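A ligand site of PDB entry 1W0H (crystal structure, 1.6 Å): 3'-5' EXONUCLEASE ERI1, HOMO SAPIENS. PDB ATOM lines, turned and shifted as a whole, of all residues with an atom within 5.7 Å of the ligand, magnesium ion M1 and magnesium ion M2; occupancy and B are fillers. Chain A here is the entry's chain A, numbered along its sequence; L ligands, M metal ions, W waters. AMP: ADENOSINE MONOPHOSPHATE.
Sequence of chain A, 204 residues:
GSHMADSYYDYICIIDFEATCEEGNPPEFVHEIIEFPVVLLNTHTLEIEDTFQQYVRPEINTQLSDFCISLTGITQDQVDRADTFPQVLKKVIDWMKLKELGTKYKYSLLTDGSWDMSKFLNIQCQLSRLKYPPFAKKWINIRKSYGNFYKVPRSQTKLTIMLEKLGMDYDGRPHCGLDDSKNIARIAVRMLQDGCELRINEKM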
ATOM      1  N   ASP A  16      23.000 -33.838 -22.808  1.00  0.00           N
ATOM      2  CA  ASP A  16      21.898 -33.682 -23.733  1.00  0.00           C
ATOM      3  C   ASP A  16      21.275 -32.302 -23.485  1.00  0.00           C
ATOM      4  O   ASP A  16      20.659 -32.077 -22.454  1.00  0.00           O
ATOM      5  CB  ASP A  16      20.873 -34.789 -23.507  1.00  0.00           C
ATOM      6  CG  ASP A  16      19.888 -34.823 -24.582  1.00  0.00           C
ATOM      7  OD1 ASP A  16      20.226 -35.303 -25.696  1.00  0.00           O
ATOM      8  OD2 ASP A  16      18.759 -34.289 -24.464  1.00  0.00           O
ATOM      9  N   PHE A  17      21.472 -31.385 -24.420  1.00  0.00           N
ATOM     10  CA  PHE A  17      21.009 -30.014 -24.269  1.00  0.00           C
ATOM     11  C   PHE A  17      19.520 -29.835 -24.543  1.00  0.00           C
ATOM     12  O   PHE A  17      18.894 -30.600 -25.308  1.00  0.00           O
ATOM     13  CB  PHE A  17      21.762 -29.074 -25.229  1.00  0.00           C
ATOM     14  CG  PHE A  17      23.237 -28.991 -24.992  1.00  0.00           C
ATOM     15  CD1 PHE A  17      23.741 -28.469 -23.798  1.00  0.00           C
ATOM     16  CD2 PHE A  17      24.133 -29.408 -25.996  1.00  0.00           C
ATOM     17  CE1 PHE A  17      25.127 -28.358 -23.605  1.00  0.00           C
ATOM     18  CE2 PHE A  17      25.522 -29.325 -25.803  1.00  0.00           C
ATOM     19  CZ  PHE A  17      26.014 -28.812 -24.607  1.00  0.00           C
ATOM     20  N   GLU A  18      18.946 -28.807 -23.907  1.00  0.00           N
ATOM     21  CA  GLU A  18      17.735 -28.194 -24.471  1.00  0.00           C
ATOM     22  C   GLU A  18      18.108 -26.834 -25.047  1.00  0.00           C
ATOM     23  O   GLU A  18      19.072 -26.183 -24.569  1.00  0.00           O
ATOM     24  CB  GLU A  18      16.595 -28.016 -23.445  1.00  0.00           C
ATOM     25  CG  GLU A  18      16.220 -29.310 -22.692  1.00  0.00           C
ATOM     26  CD  GLU A  18      15.861 -30.449 -23.622  1.00  0.00           C
ATOM     27  OE1 GLU A  18      15.205 -30.229 -24.675  1.00  0.00           O
ATOM     28  OE2 GLU A  18      16.252 -31.618 -23.309  1.00  0.00           O
ATOM     29  N   ALA A  19      17.371 -26.438 -26.074  1.00  0.00           N
ATOM     30  CA  ALA A  19      17.626 -25.172 -26.766  1.00  0.00           C
ATOM     31  C   ALA A  19      16.353 -24.423 -27.049  1.00  0.00           C
ATOM     32  O   ALA A  19      15.253 -25.020 -27.089  1.00  0.00           O
ATOM     33  CB  ALA A  19      18.363 -25.434 -28.092  1.00  0.00           C
ATOM     34  N   THR A  20      16.472 -23.119 -27.261  1.00  0.00           N
ATOM     35  CA  THR A  20      15.332 -22.350 -27.777  1.00  0.00           C
ATOM     36  C   THR A  20      14.847 -22.960 -29.092  1.00  0.00           C
ATOM     37  O   THR A  20      15.631 -23.529 -29.843  1.00  0.00           O
ATOM     38  CB  THR A  20      15.677 -20.886 -28.056  1.00  0.00           C
ATOM     39  OG1 THR A  20      16.808 -20.812 -28.932  1.00  0.00           O
ATOM     40  CG2 THR A  20      16.073 -20.171 -26.760  1.00  0.00           C
ATOM     41  N   CYS A  21      13.560 -22.824 -29.354  1.00  0.00           N
ATOM     42  CA  CYS A  21      12.989 -23.381 -30.578  1.00  0.00           C
ATOM     43  C   CYS A  21      11.660 -22.709 -30.841  1.00  0.00           C
ATOM     44  O   CYS A  21      11.108 -22.018 -29.970  1.00  0.00           O
ATOM     45  CB  CYS A  21      12.817 -24.894 -30.487  1.00  0.00           C
ATOM     46  SG  CYS A  21      11.809 -25.416 -29.049  1.00  0.00           S
ATOM     47  N   GLU A  22      11.159 -22.924 -32.051  1.00  0.00           N
ATOM     48  CA  GLU A  22       9.811 -22.515 -32.423  1.00  0.00           C
ATOM     49  C   GLU A  22       9.083 -23.707 -33.033  1.00  0.00           C
ATOM     50  O   GLU A  22       9.705 -24.654 -33.554  1.00  0.00           O
ATOM     51  CB  GLU A  22       9.850 -21.364 -33.430  1.00  0.00           C
ATOM     52  CG  GLU A  22      10.322 -20.071 -32.794  1.00  0.00           C
ATOM     53  CD  GLU A  22      10.307 -18.884 -33.751  1.00  0.00           C
ATOM     54  OE1 GLU A  22      10.421 -19.107 -34.972  1.00  0.00           O
ATOM     55  OE2 GLU A  22      10.180 -17.728 -33.278  1.00  0.00           O
ATOM     56  N   GLU A  23       7.765 -23.654 -32.938  1.00  0.00           N
ATOM     57  CA  GLU A  23       6.944 -24.721 -33.496  1.00  0.00           C
ATOM     58  C   GLU A  23       7.233 -24.848 -34.998  1.00  0.00           C
ATOM     59  O   GLU A  23       7.319 -23.835 -35.692  1.00  0.00           O
ATOM     60  CB  GLU A  23       5.462 -24.418 -33.279  1.00  0.00           C
ATOM     61  CG  GLU A  23       4.564 -25.613 -33.590  1.00  0.00           C
ATOM     62  CD  GLU A  23       3.141 -25.459 -33.090  1.00  0.00           C
ATOM     63  OE1 GLU A  23       2.755 -24.358 -32.655  1.00  0.00           O
ATOM     64  OE2 GLU A  23       2.402 -26.474 -33.135  1.00  0.00           O
ATOM     65  N   GLY A  24       7.408 -26.078 -35.463  1.00  0.00           N
ATOM     66  CA  GLY A  24       7.679 -26.315 -36.869  1.00  0.00           C
ATOM     67  C   GLY A  24       9.157 -26.310 -37.236  1.00  0.00           C
ATOM     68  O   GLY A  24       9.494 -26.582 -38.396  1.00  0.00           O
ATOM     69  N   ASN A  25      10.021 -26.001 -36.262  1.00  0.00           N
ATOM     70  CA  ASN A  25      11.463 -26.060 -36.489  1.00  0.00           C
ATOM     71  C   ASN A  25      11.912 -25.224 -37.708  1.00  0.00           C
ATOM     72  O   ASN A  25      12.582 -25.751 -38.639  1.00  0.00           O
ATOM     73  CB  ASN A  25      11.877 -27.542 -36.633  1.00  0.00           C
ATOM     74  CG  ASN A  25      13.375 -27.727 -36.706  1.00  0.00           C
ATOM     75  OD1 ASN A  25      14.126 -27.046 -36.039  1.00  0.00           O
ATOM     76  ND2 ASN A  25      13.809 -28.679 -37.529  1.00  0.00           N
ATOM     77  N   HIS A  31      19.132 -21.281 -32.901  1.00  0.00           N
ATOM     78  CA  HIS A  31      19.075 -21.958 -31.595  1.00  0.00           C
ATOM     79  C   HIS A  31      20.094 -21.420 -30.593  1.00  0.00           C
ATOM     80  O   HIS A  31      21.276 -21.212 -30.933  1.00  0.00           O
ATOM     81  CB  HIS A  31      19.371 -23.446 -31.730  1.00  0.00           C
ATOM     82  CG  HIS A  31      18.362 -24.229 -32.483  1.00  0.00           C
ATOM     83  ND1 HIS A  31      17.088 -24.473 -31.999  1.00  0.00           N
ATOM     84  CD2 HIS A  31      18.465 -24.939 -33.635  1.00  0.00           C
ATOM     85  CE1 HIS A  31      16.438 -25.260 -32.848  1.00  0.00           C
ATOM     86  NE2 HIS A  31      17.250 -25.550 -33.848  1.00  0.00           N
ATOM     87  N   PHE A  67       5.731 -22.685 -27.452  1.00  0.00           N
ATOM     88  CA  PHE A  67       6.066 -24.034 -27.856  1.00  0.00           C
ATOM     89  C   PHE A  67       7.288 -24.566 -27.071  1.00  0.00           C
ATOM     90  O   PHE A  67       7.285 -25.673 -26.562  1.00  0.00           O
ATOM     91  CB  PHE A  67       6.308 -24.116 -29.385  1.00  0.00           C
ATOM     92  CG  PHE A  67       6.723 -25.455 -29.850  1.00  0.00           C
ATOM     93  CD1 PHE A  67       5.766 -26.437 -30.150  1.00  0.00           C
ATOM     94  CD2 PHE A  67       8.086 -25.774 -29.948  1.00  0.00           C
ATOM     95  CE1 PHE A  67       6.170 -27.701 -30.560  1.00  0.00           C
ATOM     96  CE2 PHE A  67       8.481 -27.047 -30.339  1.00  0.00           C
ATOM     97  CZ  PHE A  67       7.524 -28.006 -30.651  1.00  0.00           C
ATOM     98  N   LEU A  71       7.289 -27.703 -24.601  1.00  0.00           N
ATOM     99  CA  LEU A  71       8.109 -28.862 -24.922  1.00  0.00           C
ATOM    100  C   LEU A  71       9.050 -29.246 -23.790  1.00  0.00           C
ATOM    101  O   LEU A  71       9.072 -30.406 -23.361  1.00  0.00           O
ATOM    102  CB  LEU A  71       8.911 -28.592 -26.216  1.00  0.00           C
ATOM    103  CG  LEU A  71       9.901 -29.675 -26.613  1.00  0.00           C
ATOM    104  CD1 LEU A  71       9.161 -30.897 -27.168  1.00  0.00           C
ATOM    105  CD2 LEU A  71      10.866 -29.130 -27.681  1.00  0.00           C
ATOM    106  N   THR A  72       9.808 -28.276 -23.292  1.00  0.00           N
ATOM    107  CA  THR A  72      10.895 -28.533 -22.365  1.00  0.00           C
ATOM    108  C   THR A  72      10.523 -28.386 -20.902  1.00  0.00           C
ATOM    109  O   THR A  72      11.232 -28.887 -20.029  1.00  0.00           O
ATOM    110  CB  THR A  72      12.098 -27.564 -22.616  1.00  0.00           C
ATOM    111  OG1 THR A  72      11.693 -26.220 -22.282  1.00  0.00           O
ATOM    112  CG2 THR A  72      12.491 -27.516 -24.105  1.00  0.00           C
ATOM    113  N   ASP A 112      23.017 -38.543 -27.406  1.00  0.00           N
ATOM    114  CA  ASP A 112      21.909 -39.153 -28.094  1.00  0.00           C
ATOM    115  C   ASP A 112      21.833 -38.771 -29.584  1.00  0.00           C
ATOM    116  O   ASP A 112      20.747 -38.678 -30.161  1.00  0.00           O
ATOM    117  CB  ASP A 112      20.645 -38.705 -27.356  1.00  0.00           C
ATOM    118  CG  ASP A 112      19.413 -39.368 -27.848  1.00  0.00           C
ATOM    119  OD1 ASP A 112      19.511 -40.520 -28.323  1.00  0.00           O
ATOM    120  OD2 ASP A 112      18.297 -38.809 -27.814  1.00  0.00           O
ATOM    121  N   ASP A 116      22.108 -33.461 -30.707  1.00  0.00           N
ATOM    122  CA  ASP A 116      21.683 -33.296 -29.322  1.00  0.00           C
ATOM    123  C   ASP A 116      22.736 -32.768 -28.373  1.00  0.00           C
ATOM    124  O   ASP A 116      22.413 -32.258 -27.296  1.00  0.00           O
ATOM    125  CB  ASP A 116      21.172 -34.655 -28.827  1.00  0.00           C
ATOM    126  CG  ASP A 116      19.875 -35.065 -29.494  1.00  0.00           C
ATOM    127  OD1 ASP A 116      19.892 -35.261 -30.752  1.00  0.00           O
ATOM    128  OD2 ASP A 116      18.799 -35.178 -28.838  1.00  0.00           O
ATOM    129  N   PHE A 120      24.200 -28.309 -31.312  1.00  0.00           N
ATOM    130  CA  PHE A 120      23.783 -27.171 -30.462  1.00  0.00           C
ATOM    131  C   PHE A 120      24.980 -26.449 -29.870  1.00  0.00           C
ATOM    132  O   PHE A 120      24.976 -25.213 -29.844  1.00  0.00           O
ATOM    133  CB  PHE A 120      22.843 -27.594 -29.298  1.00  0.00           C
ATOM    134  CG  PHE A 120      21.457 -27.983 -29.768  1.00  0.00           C
ATOM    135  CD1 PHE A 120      20.673 -27.115 -30.526  1.00  0.00           C
ATOM    136  CD2 PHE A 120      20.947 -29.238 -29.443  1.00  0.00           C
ATOM    137  CE1 PHE A 120      19.381 -27.466 -30.953  1.00  0.00           C
ATOM    138  CE2 PHE A 120      19.644 -29.598 -29.868  1.00  0.00           C
ATOM    139  CZ  PHE A 120      18.876 -28.714 -30.623  1.00  0.00           C
ATOM    140  N   HIS A 175      12.311 -34.259 -22.416  1.00  0.00           N
ATOM    141  CA  HIS A 175      12.729 -32.898 -22.819  1.00  0.00           C
ATOM    142  C   HIS A 175      13.103 -31.961 -21.688  1.00  0.00           C
ATOM    143  O   HIS A 175      13.325 -30.766 -21.923  1.00  0.00           O
ATOM    144  CB  HIS A 175      11.736 -32.252 -23.800  1.00  0.00           C
ATOM    145  CG  HIS A 175      11.270 -33.193 -24.869  1.00  0.00           C
ATOM    146  ND1 HIS A 175      12.092 -33.588 -25.900  1.00  0.00           N
ATOM    147  CD2 HIS A 175      10.103 -33.858 -25.026  1.00  0.00           C
ATOM    148  CE1 HIS A 175      11.435 -34.456 -26.667  1.00  0.00           C
ATOM    149  NE2 HIS A 175      10.220 -34.630 -26.157  1.00  0.00           N
ATOM    150  N   CYS A 176      13.148 -32.469 -20.457  1.00  0.00           N
ATOM    151  CA  CYS A 176      14.012 -31.906 -19.423  1.00  0.00           C
ATOM    152  C   CYS A 176      15.408 -32.443 -19.756  1.00  0.00           C
ATOM    153  O   CYS A 176      15.608 -33.664 -19.868  1.00  0.00           O
ATOM    154  CB  CYS A 176      13.561 -32.376 -18.032  1.00  0.00           C
ATOM    155  SG  CYS A 176      14.712 -32.132 -16.679  1.00  0.00           S
ATOM    156  N   GLY A 177      16.395 -31.561 -19.936  1.00  0.00           N
ATOM    157  CA  GLY A 177      17.715 -32.026 -20.350  1.00  0.00           C
ATOM    158  C   GLY A 177      18.377 -32.976 -19.355  1.00  0.00           C
ATOM    159  O   GLY A 177      19.001 -33.961 -19.765  1.00  0.00           O
ATOM    160  N   ASP A 180      16.476 -36.360 -19.627  1.00  0.00           N
ATOM    161  CA  ASP A 180      16.891 -37.085 -20.837  1.00  0.00           C
ATOM    162  C   ASP A 180      18.302 -37.639 -20.676  1.00  0.00           C
ATOM    163  O   ASP A 180      18.558 -38.777 -21.048  1.00  0.00           O
ATOM    164  CB  ASP A 180      16.875 -36.190 -22.088  1.00  0.00           C
ATOM    165  CG  ASP A 180      15.486 -35.832 -22.565  1.00  0.00           C
ATOM    166  OD1 ASP A 180      14.507 -36.544 -22.286  1.00  0.00           O
ATOM    167  OD2 ASP A 180      15.288 -34.833 -23.275  1.00  0.00           O
ATOM    168  N   ILE A 184      19.407 -41.558 -20.921  1.00  0.00           N
ATOM    169  CA  ILE A 184      20.452 -41.997 -21.821  1.00  0.00           C
ATOM    170  C   ILE A 184      21.529 -42.750 -21.024  1.00  0.00           C
ATOM    171  O   ILE A 184      22.019 -43.791 -21.476  1.00  0.00           O
ATOM    172  CB  ILE A 184      21.043 -40.767 -22.564  1.00  0.00           C
ATOM    173  CG1 ILE A 184      19.992 -40.192 -23.513  1.00  0.00           C
ATOM    174  CG2 ILE A 184      22.222 -41.187 -23.369  1.00  0.00           C
ATOM    175  CD1 ILE A 184      20.231 -38.708 -23.866  1.00  0.00           C
HETATM  176  P   AMP L   1      15.375 -33.014 -27.074  1.00  0.00           P
HETATM  177  O1P AMP L   1      16.715 -33.512 -26.607  1.00  0.00           O
HETATM  178  O2P AMP L   1      14.633 -32.329 -25.925  1.00  0.00           O
HETATM  179  O3P AMP L   1      14.471 -34.126 -27.636  1.00  0.00           O
HETATM  180  O5' AMP L   1      15.559 -31.943 -28.259  1.00  0.00           O
HETATM  181  C5' AMP L   1      16.584 -30.981 -28.063  1.00  0.00           C
HETATM  182  C4' AMP L   1      16.081 -29.641 -28.609  1.00  0.00           C
HETATM  183  O4' AMP L   1      15.686 -29.771 -29.971  1.00  0.00           O
HETATM  184  C3' AMP L   1      14.860 -29.009 -27.918  1.00  0.00           C
HETATM  185  O3' AMP L   1      15.254 -28.377 -26.734  1.00  0.00           O
HETATM  186  C2' AMP L   1      14.363 -28.103 -29.023  1.00  0.00           C
HETATM  187  O2' AMP L   1      15.168 -26.936 -29.135  1.00  0.00           O
HETATM  188  C1' AMP L   1      14.586 -28.961 -30.272  1.00  0.00           C
HETATM  189  N9  AMP L   1      13.396 -29.811 -30.491  1.00  0.00           N
HETATM  190  C8  AMP L   1      13.185 -31.089 -30.012  1.00  0.00           C
HETATM  191  N7  AMP L   1      11.967 -31.496 -30.458  1.00  0.00           N
HETATM  192  C5  AMP L   1      11.413 -30.499 -31.184  1.00  0.00           C
HETATM  193  C6  AMP L   1      10.203 -30.345 -31.862  1.00  0.00           C
HETATM  194  N6  AMP L   1       9.295 -31.328 -31.872  1.00  0.00           N
HETATM  195  N1  AMP L   1       9.935 -29.184 -32.536  1.00  0.00           N
HETATM  196  C2  AMP L   1      10.835 -28.137 -32.554  1.00  0.00           C
HETATM  197  N3  AMP L   1      12.022 -28.286 -31.883  1.00  0.00           N
HETATM  198  C4  AMP L   1      12.313 -29.430 -31.213  1.00  0.00           C
HETATM  199 MG    MG M   1      18.447 -34.606 -26.860  1.00  0.00          MG
HETATM  200 MG    MG M   2      16.691 -33.461 -24.325  1.00  0.00          MG
HETATM  201  O   HOH W   1      17.440 -36.531 -26.578  1.00  0.00           O
HETATM  202  O   HOH W   2       6.215 -31.238 -32.357  1.00  0.00           O
HETATM  203  O   HOH W   3      17.181 -32.949 -30.981  1.00  0.00           O
HETATM  204  O   HOH W   4      19.543 -32.640 -27.005  1.00  0.00           O
HETATM  205  O   HOH W   5      13.575 -34.414 -29.945  1.00  0.00           O
HETATM  206  O   HOH W   6       7.721 -28.623 -34.096  1.00  0.00           O
HETATM  207  O   HOH W   7      10.109 -33.522 -29.932  1.00  0.00           O
HETATM  208  O   HOH W   8      13.628 -30.253 -34.006  1.00  0.00           O
HETATM  209  O   HOH W   9      14.805 -36.615 -26.753  1.00  0.00           O
HETATM  210  O   HOH W  10      13.738 -26.701 -33.359  1.00  0.00           O
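Magnesium ion M2 is bound by OE2 of Glu 18 (2.1 Å), OD2 of Asp 180 (2.2 Å), OD2 of Asp 16 (2.2 Å) and O1P of the ligand (2.3 Å).
Magnesium ion M2 has four donor atoms within binding distance.
Slightly farther from magnesium ion M2 lies an oxygen (O2P) of the ligand (2.8 Å).
Water W4 bridges the backbone carbonyl oxygen of Phe 17 (2.7 Å) and the backbone carbonyl oxygen of Asp 116 (2.9 Å).
Water W10 lies within hydrogen-bond range of the side-chain amide oxygen (OD1) of Asn 25 and a nitrogen (N3) of the ligand.
Water W6 lies within hydrogen-bond range of N1 of the ligand (2.8 Å) and N of Gly 24 (2.9 Å).
Magnesium ion M1 is bound by O1P of the ligand, at 2.1 Å.
OD2 of Asp 116 binds magnesium ion M1, 2.1 Å away.
Water W1 is bound to magnesium ion M1 (2.2 Å).
Magnesium ion M1 is bound by OD1 of Asp 16 (2.2 Å).
Magnesium ion M1 is bound by water W4 (2.3 Å).
The side-chain carboxylate (OD2) of Asp 16 is bound to magnesium ion M1 (2.4 Å).
Magnesium ion M1 has six donor atoms within binding distance.
An oxygen (O3') of the ligand lies within hydrogen-bond range of the backbone NH (N) of Ala 19 (2.9 Å).
O of Ala 19 lies within hydrogen-bond range of O2' of the ligand (2.8 Å).
A ring nitrogen (ND1) of His 175 sits at hydrogen-bond distance from an oxygen (O2P) of the ligand (2.8 Å).
SG of Cys 21 lies close to O2' of the ligand, at 3.7 Å.
Merely in contact with magnesium ion M2: Phe 17 (3.7 Å).
Of the 22 residues printed, 4 come within 4 Å of magnesium ion M2.
The nearest printed residue that does not touch magnesium ion M2 is His 175 (4.3 Å).
The backbone carbonyl oxygen (O) of Asp 116 sits at hydrogen-bond distance from the backbone NH (N) of Phe 17 (3.1 Å).
The backbone NH of Gly 177 lies close to the side-chain carboxylate of Glu 18 (3.4 Å).
OD1 of Asp 180 sits at hydrogen-bond distance from N of His 175 (3.2 Å).
The backbone carbonyl oxygen (O) of Thr 20 is in hydrogen-bond range of a ring nitrogen (ND1) of His 31, 2.8 Å away.
Merely in contact with the ligand: Phe 67 (3.3 Å), Phe 120 (3.4 Å), Thr 20 (3.5 Å), Phe 17 (3.6 Å), Glu 22 (3.8 Å), Leu 71 (3.8 Å) and Thr 72 (3.9 Å).
Hydrophobic or aromatic side chains within 4 Å of the ligand: Ala 19, Phe 67, Leu 71, Phe 120 and His 175.
14 residues have an atom within 4 Å of the ligand: Asp 16, Phe 17, Glu 18, Ala 19, Thr 20, Cys 21, Glu 22, Phe 67, Leu 71, Thr 72, Asp 116, Phe 120, His 175 and Asp 180.
The nearest printed residue that does not touch the ligand is His 31 (4.2 Å).
Of the 22 residues printed, 2 come within 4 Å of magnesium ion M1.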
